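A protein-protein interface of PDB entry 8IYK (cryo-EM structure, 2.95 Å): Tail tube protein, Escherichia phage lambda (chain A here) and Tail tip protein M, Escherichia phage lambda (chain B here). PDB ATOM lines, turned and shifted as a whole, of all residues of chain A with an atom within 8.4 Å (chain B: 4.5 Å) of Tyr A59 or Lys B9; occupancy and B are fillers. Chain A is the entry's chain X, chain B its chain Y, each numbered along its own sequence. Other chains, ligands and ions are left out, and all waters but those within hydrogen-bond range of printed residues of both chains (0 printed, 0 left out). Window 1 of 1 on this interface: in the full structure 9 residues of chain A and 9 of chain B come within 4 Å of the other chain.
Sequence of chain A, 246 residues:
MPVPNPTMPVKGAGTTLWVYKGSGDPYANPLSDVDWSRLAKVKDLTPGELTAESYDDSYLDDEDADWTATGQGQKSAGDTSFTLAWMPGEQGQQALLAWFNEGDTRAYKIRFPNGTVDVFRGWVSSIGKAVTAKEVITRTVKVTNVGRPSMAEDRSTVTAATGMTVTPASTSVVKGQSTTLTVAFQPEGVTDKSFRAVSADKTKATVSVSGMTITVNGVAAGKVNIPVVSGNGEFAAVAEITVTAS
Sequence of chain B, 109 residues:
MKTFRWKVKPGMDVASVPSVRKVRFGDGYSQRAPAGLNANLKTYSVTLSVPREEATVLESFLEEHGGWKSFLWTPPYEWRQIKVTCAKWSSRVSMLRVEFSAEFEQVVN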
ATOM      1  N   TYR A  55     -22.061 -11.494  -2.748  1.00  0.00           N
ATOM      2  CA  TYR A  55     -22.290 -11.741  -4.162  1.00  0.00           C
ATOM      3  C   TYR A  55     -22.716 -13.189  -4.364  1.00  0.00           C
ATOM      4  O   TYR A  55     -22.305 -14.085  -3.622  1.00  0.00           O
ATOM      5  CB  TYR A  55     -21.037 -11.431  -4.990  1.00  0.00           C
ATOM      6  CG  TYR A  55     -19.884 -12.401  -4.819  1.00  0.00           C
ATOM      7  CD1 TYR A  55     -19.841 -13.598  -5.523  1.00  0.00           C
ATOM      8  CD2 TYR A  55     -18.828 -12.110  -3.969  1.00  0.00           C
ATOM      9  CE1 TYR A  55     -18.794 -14.481  -5.374  1.00  0.00           C
ATOM     10  CE2 TYR A  55     -17.772 -12.989  -3.817  1.00  0.00           C
ATOM     11  CZ  TYR A  55     -17.763 -14.172  -4.520  1.00  0.00           C
ATOM     12  OH  TYR A  55     -16.716 -15.050  -4.372  1.00  0.00           O
ATOM     13  N   ASP A  56     -23.552 -13.409  -5.375  1.00  0.00           N
ATOM     14  CA  ASP A  56     -24.016 -14.755  -5.678  1.00  0.00           C
ATOM     15  C   ASP A  56     -22.874 -15.601  -6.228  1.00  0.00           C
ATOM     16  O   ASP A  56     -22.076 -15.140  -7.048  1.00  0.00           O
ATOM     17  CB  ASP A  56     -25.165 -14.707  -6.682  1.00  0.00           C
ATOM     18  CG  ASP A  56     -26.365 -15.507  -6.226  1.00  0.00           C
ATOM     19  OD1 ASP A  56     -26.170 -16.607  -5.670  1.00  0.00           O
ATOM     20  OD2 ASP A  56     -27.506 -15.034  -6.420  1.00  0.00           O
ATOM     21  N   ASP A  57     -22.804 -16.854  -5.778  1.00  0.00           N
ATOM     22  CA  ASP A  57     -21.713 -17.749  -6.143  1.00  0.00           C
ATOM     23  C   ASP A  57     -22.230 -19.112  -6.581  1.00  0.00           C
ATOM     24  O   ASP A  57     -21.579 -20.133  -6.347  1.00  0.00           O
ATOM     25  CB  ASP A  57     -20.727 -17.905  -4.986  1.00  0.00           C
ATOM     26  CG  ASP A  57     -19.307 -18.124  -5.457  1.00  0.00           C
ATOM     27  OD1 ASP A  57     -18.900 -17.470  -6.439  1.00  0.00           O
ATOM     28  OD2 ASP A  57     -18.598 -18.953  -4.849  1.00  0.00           O
ATOM     29  N   SER A  58     -23.395 -19.149  -7.219  1.00  0.00           N
ATOM     30  CA  SER A  58     -23.993 -20.388  -7.698  1.00  0.00           C
ATOM     31  C   SER A  58     -24.019 -20.360  -9.220  1.00  0.00           C
ATOM     32  O   SER A  58     -24.568 -19.427  -9.813  1.00  0.00           O
ATOM     33  CB  SER A  58     -25.402 -20.569  -7.137  1.00  0.00           C
ATOM     34  OG  SER A  58     -26.147 -19.370  -7.241  1.00  0.00           O
ATOM     35  N   TYR A  59     -23.436 -21.381  -9.842  1.00  0.00           N
ATOM     36  CA  TYR A  59     -23.344 -21.478 -11.290  1.00  0.00           C
ATOM     37  C   TYR A  59     -24.115 -22.695 -11.780  1.00  0.00           C
ATOM     38  O   TYR A  59     -24.295 -23.671 -11.049  1.00  0.00           O
ATOM     39  CB  TYR A  59     -21.884 -21.560 -11.749  1.00  0.00           C
ATOM     40  CG  TYR A  59     -21.003 -20.473 -11.179  1.00  0.00           C
ATOM     41  CD1 TYR A  59     -21.087 -19.172 -11.649  1.00  0.00           C
ATOM     42  CD2 TYR A  59     -20.090 -20.747 -10.172  1.00  0.00           C
ATOM     43  CE1 TYR A  59     -20.286 -18.174 -11.135  1.00  0.00           C
ATOM     44  CE2 TYR A  59     -19.286 -19.756  -9.651  1.00  0.00           C
ATOM     45  CZ  TYR A  59     -19.388 -18.472 -10.136  1.00  0.00           C
ATOM     46  OH  TYR A  59     -18.588 -17.479  -9.620  1.00  0.00           O
ATOM     47  N   LEU A  60     -24.576 -22.621 -13.032  1.00  0.00           N
ATOM     48  CA  LEU A  60     -25.416 -23.684 -13.579  1.00  0.00           C
ATOM     49  C   LEU A  60     -24.659 -25.001 -13.686  1.00  0.00           C
ATOM     50  O   LEU A  60     -25.212 -26.066 -13.391  1.00  0.00           O
ATOM     51  CB  LEU A  60     -25.957 -23.273 -14.947  1.00  0.00           C
ATOM     52  CG  LEU A  60     -27.192 -22.375 -14.964  1.00  0.00           C
ATOM     53  CD1 LEU A  60     -27.848 -22.421 -16.327  1.00  0.00           C
ATOM     54  CD2 LEU A  60     -28.170 -22.786 -13.881  1.00  0.00           C
ATOM     55  N   ASP A  61     -23.396 -24.953 -14.116  1.00  0.00           N
ATOM     56  CA  ASP A  61     -22.612 -26.170 -14.288  1.00  0.00           C
ATOM     57  C   ASP A  61     -22.261 -26.843 -12.970  1.00  0.00           C
ATOM     58  O   ASP A  61     -21.808 -27.991 -12.987  1.00  0.00           O
ATOM     59  CB  ASP A  61     -21.324 -25.866 -15.055  1.00  0.00           C
ATOM     60  CG  ASP A  61     -21.416 -24.597 -15.873  1.00  0.00           C
ATOM     61  OD1 ASP A  61     -21.842 -23.562 -15.322  1.00  0.00           O
ATOM     62  OD2 ASP A  61     -21.053 -24.632 -17.067  1.00  0.00           O
ATOM     63  N   ASP A  62     -22.447 -26.163 -11.843  1.00  0.00           N
ATOM     64  CA  ASP A  62     -22.041 -26.708 -10.557  1.00  0.00           C
ATOM     65  C   ASP A  62     -22.867 -27.933 -10.189  1.00  0.00           C
ATOM     66  O   ASP A  62     -24.080 -27.976 -10.409  1.00  0.00           O
ATOM     67  CB  ASP A  62     -22.184 -25.647  -9.466  1.00  0.00           C
ATOM     68  CG  ASP A  62     -20.950 -24.785  -9.326  1.00  0.00           C
ATOM     69  OD1 ASP A  62     -20.000 -24.975 -10.113  1.00  0.00           O
ATOM     70  OD2 ASP A  62     -20.930 -23.918  -8.429  1.00  0.00           O
ATOM     71  N   GLU A  63     -22.197 -28.935  -9.630  1.00  0.00           N
ATOM     72  CA  GLU A  63     -22.892 -30.026  -8.970  1.00  0.00           C
ATOM     73  C   GLU A  63     -23.327 -29.587  -7.575  1.00  0.00           C
ATOM     74  O   GLU A  63     -22.874 -28.567  -7.047  1.00  0.00           O
ATOM     75  CB  GLU A  63     -22.009 -31.275  -8.894  1.00  0.00           C
ATOM     76  CG  GLU A  63     -21.861 -32.094 -10.188  1.00  0.00           C
ATOM     77  CD  GLU A  63     -21.557 -31.281 -11.442  1.00  0.00           C
ATOM     78  OE1 GLU A  63     -21.744 -31.826 -12.550  1.00  0.00           O
ATOM     79  OE2 GLU A  63     -21.076 -30.134 -11.335  1.00  0.00           O
ATOM     80  N   ASP A  64     -24.220 -30.375  -6.974  1.00  0.00           N
ATOM     81  CA  ASP A  64     -24.832 -30.039  -5.690  1.00  0.00           C
ATOM     82  C   ASP A  64     -25.551 -28.691  -5.780  1.00  0.00           C
ATOM     83  O   ASP A  64     -25.187 -27.708  -5.132  1.00  0.00           O
ATOM     84  CB  ASP A  64     -23.796 -30.052  -4.559  1.00  0.00           C
ATOM     85  CG  ASP A  64     -24.413 -29.780  -3.200  1.00  0.00           C
ATOM     86  OD1 ASP A  64     -25.269 -30.579  -2.766  1.00  0.00           O
ATOM     87  OD2 ASP A  64     -24.047 -28.766  -2.569  1.00  0.00           O
ATOM     88  N   ALA A  65     -26.577 -28.662  -6.625  1.00  0.00           N
ATOM     89  CA  ALA A  65     -27.384 -27.467  -6.823  1.00  0.00           C
ATOM     90  C   ALA A  65     -28.459 -27.296  -5.761  1.00  0.00           C
ATOM     91  O   ALA A  65     -29.197 -26.306  -5.801  1.00  0.00           O
ATOM     92  CB  ALA A  65     -28.031 -27.499  -8.208  1.00  0.00           C
ATOM     93  N   TRP A  67     -28.123 -26.689  -2.555  1.00  0.00           N
ATOM     94  CA  TRP A  67     -27.772 -25.738  -1.509  1.00  0.00           C
ATOM     95  C   TRP A  67     -27.206 -24.474  -2.135  1.00  0.00           C
ATOM     96  O   TRP A  67     -26.339 -24.546  -3.012  1.00  0.00           O
ATOM     97  CB  TRP A  67     -26.760 -26.345  -0.536  1.00  0.00           C
ATOM     98  CG  TRP A  67     -27.348 -27.377   0.369  1.00  0.00           C
ATOM     99  CD1 TRP A  67     -27.488 -28.706   0.110  1.00  0.00           C
ATOM    100  CD2 TRP A  67     -27.879 -27.164   1.681  1.00  0.00           C
ATOM    101  NE1 TRP A  67     -28.072 -29.338   1.180  1.00  0.00           N
ATOM    102  CE2 TRP A  67     -28.323 -28.412   2.157  1.00  0.00           C
ATOM    103  CE3 TRP A  67     -28.024 -26.041   2.499  1.00  0.00           C
ATOM    104  CZ2 TRP A  67     -28.898 -28.569   3.413  1.00  0.00           C
ATOM    105  CZ3 TRP A  67     -28.596 -26.199   3.746  1.00  0.00           C
ATOM    106  CH2 TRP A  67     -29.026 -27.452   4.191  1.00  0.00           C
ATOM    107  N   ALA A  69     -25.088 -20.961  -2.500  1.00  0.00           N
ATOM    108  CA  ALA A  69     -23.744 -20.526  -2.156  1.00  0.00           C
ATOM    109  C   ALA A  69     -23.600 -19.042  -2.459  1.00  0.00           C
ATOM    110  O   ALA A  69     -24.225 -18.519  -3.384  1.00  0.00           O
ATOM    111  CB  ALA A  69     -22.682 -21.322  -2.920  1.00  0.00           C
ATOM    112  N   THR A  70     -22.767 -18.369  -1.670  1.00  0.00           N
ATOM    113  CA  THR A  70     -22.527 -16.940  -1.827  1.00  0.00           C
ATOM    114  C   THR A  70     -21.037 -16.681  -1.633  1.00  0.00           C
ATOM    115  O   THR A  70     -20.233 -17.610  -1.520  1.00  0.00           O
ATOM    116  CB  THR A  70     -23.375 -16.124  -0.843  1.00  0.00           C
ATOM    117  OG1 THR A  70     -23.380 -16.766   0.436  1.00  0.00           O
ATOM    118  CG2 THR A  70     -24.801 -15.995  -1.341  1.00  0.00           C
ATOM    119  N   LYS B   7     -18.159 -20.371 -16.325  1.00  0.00           N
ATOM    120  CA  LYS B   7     -19.437 -20.962 -15.948  1.00  0.00           C
ATOM    121  C   LYS B   7     -20.513 -19.890 -15.849  1.00  0.00           C
ATOM    122  O   LYS B   7     -20.235 -18.740 -15.499  1.00  0.00           O
ATOM    123  CB  LYS B   7     -19.310 -21.712 -14.616  1.00  0.00           C
ATOM    124  CG  LYS B   7     -17.890 -22.177 -14.318  1.00  0.00           C
ATOM    125  CD  LYS B   7     -17.865 -23.424 -13.458  1.00  0.00           C
ATOM    126  CE  LYS B   7     -18.335 -23.129 -12.049  1.00  0.00           C
ATOM    127  NZ  LYS B   7     -17.363 -22.282 -11.304  1.00  0.00           N
ATOM    128  N   VAL B   8     -21.754 -20.286 -16.131  1.00  0.00           N
ATOM    129  CA  VAL B   8     -22.885 -19.367 -16.244  1.00  0.00           C
ATOM    130  C   VAL B   8     -23.798 -19.545 -15.036  1.00  0.00           C
ATOM    131  O   VAL B   8     -24.258 -20.658 -14.750  1.00  0.00           O
ATOM    132  CB  VAL B   8     -23.643 -19.584 -17.565  1.00  0.00           C
ATOM    133  CG1 VAL B   8     -22.771 -19.168 -18.718  1.00  0.00           C
ATOM    134  CG2 VAL B   8     -24.033 -21.039 -17.736  1.00  0.00           C
ATOM    135  N   LYS B   9     -24.029 -18.455 -14.305  1.00  0.00           N
ATOM    136  CA  LYS B   9     -24.712 -18.529 -13.016  1.00  0.00           C
ATOM    137  C   LYS B   9     -26.246 -18.569 -13.023  1.00  0.00           C
ATOM    138  O   LYS B   9     -26.827 -19.496 -12.446  1.00  0.00           O
ATOM    139  CB  LYS B   9     -24.211 -17.384 -12.121  1.00  0.00           C
ATOM    140  CG  LYS B   9     -24.509 -15.964 -12.576  1.00  0.00           C
ATOM    141  CD  LYS B   9     -23.395 -15.005 -12.208  1.00  0.00           C
ATOM    142  CE  LYS B   9     -22.752 -15.358 -10.874  1.00  0.00           C
ATOM    143  NZ  LYS B   9     -23.736 -15.391  -9.753  1.00  0.00           N
ATOM    144  N   PRO B  10     -26.949 -17.606 -13.643  1.00  0.00           N
ATOM    145  CA  PRO B  10     -28.306 -17.300 -13.171  1.00  0.00           C
ATOM    146  C   PRO B  10     -29.420 -18.136 -13.778  1.00  0.00           C
ATOM    147  O   PRO B  10     -30.479 -18.300 -13.165  1.00  0.00           O
ATOM    148  CB  PRO B  10     -28.463 -15.826 -13.558  1.00  0.00           C
ATOM    149  CG  PRO B  10     -27.649 -15.700 -14.818  1.00  0.00           C
ATOM    150  CD  PRO B  10     -26.666 -16.868 -14.888  1.00  0.00           C
ATOM    151  N   GLY B  11     -29.200 -18.673 -14.968  1.00  0.00           N
ATOM    152  CA  GLY B  11     -30.295 -19.176 -15.766  1.00  0.00           C
ATOM    153  C   GLY B  11     -30.405 -18.426 -17.072  1.00  0.00           C
ATOM    154  O   GLY B  11     -30.813 -17.260 -17.111  1.00  0.00           O
ATOM    155  N   THR B  47     -24.423 -15.405 -19.391  1.00  0.00           N
ATOM    156  CA  THR B  47     -23.941 -14.312 -18.557  1.00  0.00           C
ATOM    157  C   THR B  47     -23.004 -14.851 -17.487  1.00  0.00           C
ATOM    158  O   THR B  47     -23.377 -15.736 -16.712  1.00  0.00           O
ATOM    159  CB  THR B  47     -25.106 -13.545 -17.926  1.00  0.00           C
ATOM    160  OG1 THR B  47     -24.679 -12.935 -16.701  1.00  0.00           O
ATOM    161  CG2 THR B  47     -26.272 -14.464 -17.675  1.00  0.00           C
ATOM    162  N   SER B  49     -20.056 -13.968 -14.323  1.00  0.00           N
ATOM    163  CA  SER B  49     -19.562 -13.021 -13.332  1.00  0.00           C
ATOM    164  C   SER B  49     -18.175 -13.470 -12.911  1.00  0.00           C
ATOM    165  O   SER B  49     -17.985 -14.631 -12.536  1.00  0.00           O
ATOM    166  CB  SER B  49     -20.487 -12.934 -12.118  1.00  0.00           C
ATOM    167  OG  SER B  49     -19.770 -12.538 -10.964  1.00  0.00           O
ATOM    168  N   ARG B  97     -15.824  -6.942  -9.139  1.00  0.00           N
ATOM    169  CA  ARG B  97     -16.168  -7.979 -10.097  1.00  0.00           C
ATOM    170  C   ARG B  97     -16.583  -7.340 -11.413  1.00  0.00           C
ATOM    171  O   ARG B  97     -16.904  -6.152 -11.477  1.00  0.00           O
ATOM    172  CB  ARG B  97     -17.292  -8.880  -9.573  1.00  0.00           C
ATOM    173  CG  ARG B  97     -16.880  -9.780  -8.424  1.00  0.00           C
ATOM    174  CD  ARG B  97     -17.716 -11.043  -8.390  1.00  0.00           C
ATOM    175  NE  ARG B  97     -16.893 -12.228  -8.191  1.00  0.00           N
ATOM    176  CZ  ARG B  97     -17.227 -13.446  -8.594  1.00  0.00           C
ATOM    177  NH1 ARG B  97     -18.368 -13.677  -9.221  1.00  0.00           N
ATOM    178  NH2 ARG B  97     -16.396 -14.457  -8.362  1.00  0.00           N
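N of Val B8 lies within hydrogen-bond range of OD1 of Asp A61, at 3.4 Å. The backbone carbonyl oxygen (O) of Asp A56 lies within hydrogen-bond range of the side-chain amino group (NZ) of Lys B9, at 3.2 Å. The backbone carbonyl oxygen (O) of Ser A58 lies close to the backbone carbonyl oxygen (O) of Lys B9. The backbone carbonyl oxygen of Val B8 sits at hydrogen-bond distance from the backbone NH of Leu A60 (2.6 Å). OD1 of Asp A62 lies within salt-bridge range of NZ of Lys B7, 3.95 Å away.
The side-chain hydroxyl (OG) of Ser A58 is in hydrogen-bond range of the side-chain carboxylate (OD1) of Asp A56 (3.2 Å). OH of Tyr A59 sits at hydrogen-bond distance from OD1 of Asp A57 (3.2 Å). The side-chain hydroxyl of Ser B49 is in hydrogen-bond range of the guanidinium group of Arg B97.
Among the printed residues, pairs that only touch across the chains: Asp A61 with Lys B7, Tyr A59 with Lys B7, Tyr A59 with Val B8, Tyr A59 with Lys B9, Tyr A55 with Arg B97, Tyr A59 with Arg B97 and Leu A60 with Lys B9.
Printed residues of chain B within 4 Å of Tyr A55: Arg B97. Of the printed residues of chain B, Ser A58 touches Lys B9 (3.1 Å). Of chain B, only Lys B7 (3.3 Å), Val B8 (3.6 Å), Lys B9 (3.6 Å) and Arg B97 (3.8 Å) come within 4 Å of Tyr A59. Of the printed residues of chain B, Asp A61 touches Lys B7 and Val B8. Glu A63 touches none of the printed residues of chain B. Trp A67 touches none of the printed residues of chain B. Printed residues of chain A within 4 Å of Val B8: Tyr A59, Leu A60 and Asp A61. Of chain A, only Asp A56 (3.2 Å), Ser A58 (3.1 Å), Tyr A59 (3.6 Å) and Leu A60 (3.8 Å) come within 4 Å of Lys B9. No residue of chain A comes within 4 Å of Pro B10. Printed residues of chain A within 4 Å of Arg B97: Tyr A55 (3.7 Å) and Tyr A59 (3.8 Å). The nearest residue of chain A that does not touch Lys B9 is Asp A57 (4.3 Å). The nearest printed residue of chain B that does not touch Tyr A55 is Ser B49 (5.5 Å).
Hydrophobic or aromatic side chains of chain A within 4 Å of the printed part of chain B: Tyr A55, Tyr A59 and Leu A60. Among the printed residues, Asp or Glu carboxylates within 4 Å of a Lys or Arg side-chain nitrogen of the other chain: Asp A62 with Lys B7.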
